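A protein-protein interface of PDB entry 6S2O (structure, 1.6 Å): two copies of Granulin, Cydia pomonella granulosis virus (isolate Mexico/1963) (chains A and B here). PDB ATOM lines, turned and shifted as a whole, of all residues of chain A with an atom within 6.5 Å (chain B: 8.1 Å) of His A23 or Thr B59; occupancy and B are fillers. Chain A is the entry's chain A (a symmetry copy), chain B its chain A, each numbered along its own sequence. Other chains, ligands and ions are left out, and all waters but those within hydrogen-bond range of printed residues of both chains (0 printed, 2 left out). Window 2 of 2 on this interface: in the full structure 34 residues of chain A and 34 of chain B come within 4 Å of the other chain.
No position is printed for both chains. Of the 7 pairs that touch across the chains among the printed residues, none has its exchanged pair printed and touching as well.
His A23 touches just these residues of chain B: Thr B59 (3.6 Å) and Glu B60 (2.7 Å). Of the printed residues of chain B, Asn A21 touches Met B119. Printed residues of chain B within 4 Å of Lys A25: Met B57 (3.2 Å) and Val B58 (2.9 Å). Cys A17 touches none of the printed residues of chain B. Pro B66 touches none of the printed residues of chain A. The nearest residue of chain B that does not touch His A23 is Val B58 (4.1 Å).
Among the printed residues, merely in contact across the chains: Lys A25 with Met B57, Leu A24 with Val B58, His A23 with Thr B59 and Leu A24 with Met B57.
The side-chain amide nitrogen (ND2) of Asn A21 sits close to the backbone carbonyl oxygen (O) of Met B119, at 3.1 Å. O of His A23 lies close to N of Glu B60 (2.7 Å). The backbone NH (N) of Val B58 sits close to the backbone carbonyl oxygen (O) of Lys A25, 2.9 Å away.
Hydrophobic or aromatic side chains of chain B that line the printed part of chain A: Met B57 and Val B58. Of the 9 printed residues of chain A, 4 touch a printed residue of chain B. Hydrophobic or aromatic side chains of chain A within 4 Å of the printed part of chain B: His A23 and Leu A24. Among the printed residues, 7 pairs touch across the chains. Among the printed residues, no Asp or Glu carboxylate lies within 4 Å of a Lys or Arg side-chain nitrogen of the other chain.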
ATOM      1  N   SER A  16     -25.063 -14.919   7.717  1.00  0.00           N
ATOM      2  CA  SER A  16     -25.532 -15.611   6.519  1.00  0.00           C
ATOM      3  C   SER A  16     -26.249 -16.892   6.923  1.00  0.00           C
ATOM      4  O   SER A  16     -26.039 -17.424   8.023  1.00  0.00           O
ATOM      5  CB  SER A  16     -24.359 -15.921   5.578  1.00  0.00           C
ATOM      6  OG  SER A  16     -23.390 -16.725   6.260  1.00  0.00           O
ATOM      7  N   CYS A  17     -27.116 -17.390   6.043  1.00  0.00           N
ATOM      8  CA  CYS A  17     -27.729 -18.692   6.305  1.00  0.00           C
ATOM      9  C   CYS A  17     -28.142 -19.293   4.976  1.00  0.00           C
ATOM     10  O   CYS A  17     -28.084 -18.632   3.940  1.00  0.00           O
ATOM     11  CB  CYS A  17     -28.913 -18.596   7.285  1.00  0.00           C
ATOM     12  SG  CYS A  17     -30.379 -17.683   6.709  1.00  0.00           S
ATOM     13  N   VAL A  18     -28.523 -20.570   4.997  1.00  0.00           N
ATOM     14  CA  VAL A  18     -28.802 -21.291   3.745  1.00  0.00           C
ATOM     15  C   VAL A  18     -30.188 -21.913   3.828  1.00  0.00           C
ATOM     16  O   VAL A  18     -30.477 -22.658   4.769  1.00  0.00           O
ATOM     17  CB  VAL A  18     -27.748 -22.393   3.459  1.00  0.00           C
ATOM     18  CG1 VAL A  18     -28.058 -23.162   2.156  1.00  0.00           C
ATOM     19  CG2 VAL A  18     -26.361 -21.811   3.376  1.00  0.00           C
ATOM     20  N   ILE A  19     -31.025 -21.661   2.815  1.00  0.00           N
ATOM     21  CA  ILE A  19     -32.405 -22.141   2.793  1.00  0.00           C
ATOM     22  C   ILE A  19     -32.650 -22.736   1.406  1.00  0.00           C
ATOM     23  O   ILE A  19     -32.621 -22.008   0.408  1.00  0.00           O
ATOM     24  CB  ILE A  19     -33.422 -21.025   3.098  1.00  0.00           C
ATOM     25  CG1 ILE A  19     -33.196 -20.437   4.502  1.00  0.00           C
ATOM     26  CG2 ILE A  19     -34.836 -21.554   2.962  1.00  0.00           C
ATOM     27  CD1 ILE A  19     -34.152 -19.246   4.864  1.00  0.00           C
ATOM     28  N   ASN A  21     -30.757 -24.561  -0.522  1.00  0.00           N
ATOM     29  CA  ASN A  21     -29.569 -24.321  -1.338  1.00  0.00           C
ATOM     30  C   ASN A  21     -29.263 -22.841  -1.538  1.00  0.00           C
ATOM     31  O   ASN A  21     -28.161 -22.502  -1.984  1.00  0.00           O
ATOM     32  CB  ASN A  21     -29.668 -24.988  -2.720  1.00  0.00           C
ATOM     33  CG  ASN A  21     -29.854 -26.472  -2.635  1.00  0.00           C
ATOM     34  OD1 ASN A  21     -29.072 -27.174  -1.994  1.00  0.00           O
ATOM     35  ND2 ASN A  21     -30.892 -26.975  -3.297  1.00  0.00           N
ATOM     36  N   HIS A  22     -30.214 -21.959  -1.243  1.00  0.00           N
ATOM     37  CA  HIS A  22     -30.038 -20.535  -1.500  1.00  0.00           C
ATOM     38  C   HIS A  22     -29.424 -19.837  -0.294  1.00  0.00           C
ATOM     39  O   HIS A  22     -29.774 -20.127   0.853  1.00  0.00           O
ATOM     40  CB  HIS A  22     -31.389 -19.923  -1.861  1.00  0.00           C
ATOM     41  CG  HIS A  22     -32.040 -20.627  -3.005  1.00  0.00           C
ATOM     42  ND1 HIS A  22     -31.363 -20.923  -4.170  1.00  0.00           N
ATOM     43  CD2 HIS A  22     -33.286 -21.134  -3.155  1.00  0.00           C
ATOM     44  CE1 HIS A  22     -32.168 -21.571  -4.993  1.00  0.00           C
ATOM     45  NE2 HIS A  22     -33.344 -21.707  -4.402  1.00  0.00           N
ATOM     46  N   HIS A  23     -28.486 -18.936  -0.566  1.00  0.00           N
ATOM     47  CA  HIS A  23     -27.691 -18.255   0.453  1.00  0.00           C
ATOM     48  C   HIS A  23     -28.356 -16.915   0.746  1.00  0.00           C
ATOM     49  O   HIS A  23     -28.635 -16.158  -0.187  1.00  0.00           O
ATOM     50  CB  HIS A  23     -26.266 -18.032  -0.068  1.00  0.00           C
ATOM     51  CG  HIS A  23     -25.226 -17.934   0.994  1.00  0.00           C
ATOM     52  ND1 HIS A  23     -23.931 -17.552   0.719  1.00  0.00           N
ATOM     53  CD2 HIS A  23     -25.259 -18.241   2.312  1.00  0.00           C
ATOM     54  CE1 HIS A  23     -23.219 -17.595   1.829  1.00  0.00           C
ATOM     55  NE2 HIS A  23     -24.001 -18.009   2.811  1.00  0.00           N
ATOM     56  N   LEU A  24     -28.619 -16.623   2.020  1.00  0.00           N
ATOM     57  CA  LEU A  24     -29.146 -15.332   2.430  1.00  0.00           C
ATOM     58  C   LEU A  24     -28.082 -14.610   3.250  1.00  0.00           C
ATOM     59  O   LEU A  24     -27.299 -15.239   3.966  1.00  0.00           O
ATOM     60  CB  LEU A  24     -30.439 -15.490   3.244  1.00  0.00           C
ATOM     61  CG  LEU A  24     -31.767 -15.811   2.534  1.00  0.00           C
ATOM     62  CD1 LEU A  24     -31.806 -17.232   2.010  1.00  0.00           C
ATOM     63  CD2 LEU A  24     -32.975 -15.568   3.460  1.00  0.00           C
ATOM     64  N   LYS A  25     -28.045 -13.291   3.123  1.00  0.00           N
ATOM     65  CA  LYS A  25     -27.087 -12.457   3.827  1.00  0.00           C
ATOM     66  C   LYS A  25     -27.790 -11.205   4.361  1.00  0.00           C
ATOM     67  O   LYS A  25     -28.691 -10.672   3.716  1.00  0.00           O
ATOM     68  CB  LYS A  25     -25.911 -12.086   2.889  1.00  0.00           C
ATOM     69  CG  LYS A  25     -24.844 -11.269   3.584  1.00  0.00           C
ATOM     70  CD  LYS A  25     -23.611 -11.111   2.682  1.00  0.00           C
ATOM     71  CE  LYS A  25     -22.624 -10.094   3.239  1.00  0.00           C
ATOM     72  NZ  LYS A  25     -21.579  -9.875   2.212  1.00  0.00           N
ATOM     73  N   MET B  57     -32.753  -9.584   5.409  1.00  0.00           N
ATOM     74  CA  MET B  57     -31.774 -10.302   4.597  1.00  0.00           C
ATOM     75  C   MET B  57     -32.197 -10.305   3.132  1.00  0.00           C
ATOM     76  O   MET B  57     -33.385 -10.295   2.828  1.00  0.00           O
ATOM     77  CB  MET B  57     -31.634 -11.754   5.071  1.00  0.00           C
ATOM     78  CG  MET B  57     -31.289 -11.875   6.534  1.00  0.00           C
ATOM     79  SD  MET B  57     -30.941 -13.572   7.055  1.00  0.00           S
ATOM     80  CE  MET B  57     -29.144 -13.520   7.011  1.00  0.00           C
ATOM     81  N   VAL B  58     -31.210 -10.377   2.222  1.00  0.00           N
ATOM     82  CA  VAL B  58     -31.452 -10.540   0.782  1.00  0.00           C
ATOM     83  C   VAL B  58     -30.896 -11.899   0.327  1.00  0.00           C
ATOM     84  O   VAL B  58     -30.096 -12.528   1.006  1.00  0.00           O
ATOM     85  CB  VAL B  58     -30.813  -9.398  -0.047  1.00  0.00           C
ATOM     86  CG1 VAL B  58     -31.581  -8.102   0.151  1.00  0.00           C
ATOM     87  CG2 VAL B  58     -29.346  -9.216   0.315  1.00  0.00           C
ATOM     88  N   THR B  59     -31.309 -12.346  -0.858  1.00  0.00           N
ATOM     89  CA  THR B  59     -30.928 -13.675  -1.342  1.00  0.00           C
ATOM     90  C   THR B  59     -29.807 -13.568  -2.375  1.00  0.00           C
ATOM     91  O   THR B  59     -29.884 -12.751  -3.296  1.00  0.00           O
ATOM     92  CB  THR B  59     -32.137 -14.391  -1.957  1.00  0.00           C
ATOM     93  OG1 THR B  59     -33.210 -14.426  -0.998  1.00  0.00           O
ATOM     94  CG2 THR B  59     -31.787 -15.816  -2.373  1.00  0.00           C
ATOM     95  N   GLU B  60     -28.756 -14.385  -2.232  1.00  0.00           N
ATOM     96  CA  GLU B  60     -27.696 -14.345  -3.241  1.00  0.00           C
ATOM     97  C   GLU B  60     -28.207 -14.864  -4.590  1.00  0.00           C
ATOM     98  O   GLU B  60     -28.950 -15.841  -4.654  1.00  0.00           O
ATOM     99  CB  GLU B  60     -26.481 -15.164  -2.774  1.00  0.00           C
ATOM    100  CG  GLU B  60     -25.248 -14.970  -3.663  1.00  0.00           C
ATOM    101  CD  GLU B  60     -23.935 -15.423  -3.014  1.00  0.00           C
ATOM    102  OE1 GLU B  60     -23.970 -15.970  -1.893  1.00  0.00           O
ATOM    103  OE2 GLU B  60     -22.861 -15.217  -3.640  1.00  0.00           O
ATOM    104  N   ASP B  61     -27.830 -14.174  -5.674  1.00  0.00           N
ATOM    105  CA  ASP B  61     -28.175 -14.584  -7.039  1.00  0.00           C
ATOM    106  C   ASP B  61     -27.721 -16.031  -7.267  1.00  0.00           C
ATOM    107  O   ASP B  61     -26.522 -16.317  -7.124  1.00  0.00           O
ATOM    108  CB  ASP B  61     -27.460 -13.615  -8.006  1.00  0.00           C
ATOM    109  CG  ASP B  61     -27.684 -13.936  -9.491  1.00  0.00           C
ATOM    110  OD1 ASP B  61     -27.697 -15.119  -9.906  1.00  0.00           O
ATOM    111  OD2 ASP B  61     -27.802 -12.968 -10.275  1.00  0.00           O
ATOM    112  N   PRO B  62     -28.626 -16.962  -7.581  1.00  0.00           N
ATOM    113  CA  PRO B  62     -28.204 -18.374  -7.714  1.00  0.00           C
ATOM    114  C   PRO B  62     -27.122 -18.610  -8.759  1.00  0.00           C
ATOM    115  O   PRO B  62     -26.320 -19.542  -8.618  1.00  0.00           O
ATOM    116  CB  PRO B  62     -29.503 -19.101  -8.102  1.00  0.00           C
ATOM    117  CG  PRO B  62     -30.603 -18.246  -7.558  1.00  0.00           C
ATOM    118  CD  PRO B  62     -30.088 -16.807  -7.647  1.00  0.00           C
ATOM    119  N   GLY B  65     -23.719 -17.259  -7.559  1.00  0.00           N
ATOM    120  CA  GLY B  65     -23.416 -17.688  -6.220  1.00  0.00           C
ATOM    121  C   GLY B  65     -22.856 -19.088  -6.218  1.00  0.00           C
ATOM    122  O   GLY B  65     -22.309 -19.568  -7.208  1.00  0.00           O
ATOM    123  N   PRO B  66     -23.057 -19.782  -5.113  1.00  0.00           N
ATOM    124  CA  PRO B  66     -22.397 -21.085  -4.907  1.00  0.00           C
ATOM    125  C   PRO B  66     -22.840 -22.133  -5.921  1.00  0.00           C
ATOM    126  O   PRO B  66     -23.965 -22.088  -6.435  1.00  0.00           O
ATOM    127  CB  PRO B  66     -22.831 -21.467  -3.495  1.00  0.00           C
ATOM    128  CG  PRO B  66     -22.988 -20.107  -2.796  1.00  0.00           C
ATOM    129  CD  PRO B  66     -23.665 -19.240  -3.890  1.00  0.00           C
ATOM    130  N   MET B 119     -27.734 -29.365  -7.349  1.00  0.00           N
ATOM    131  CA  MET B 119     -28.452 -28.559  -6.362  1.00  0.00           C
ATOM    132  C   MET B 119     -29.847 -28.179  -6.857  1.00  0.00           C
ATOM    133  O   MET B 119     -30.825 -28.237  -6.098  1.00  0.00           O
ATOM    134  CB  MET B 119     -27.672 -27.284  -6.049  1.00  0.00           C
ATOM    135  CG  MET B 119     -26.255 -27.560  -5.613  1.00  0.00           C
ATOM    136  SD  MET B 119     -25.101 -26.188  -5.795  1.00  0.00           S
ATOM    137  CE  MET B 119     -25.991 -24.849  -4.999  1.00  0.00           C
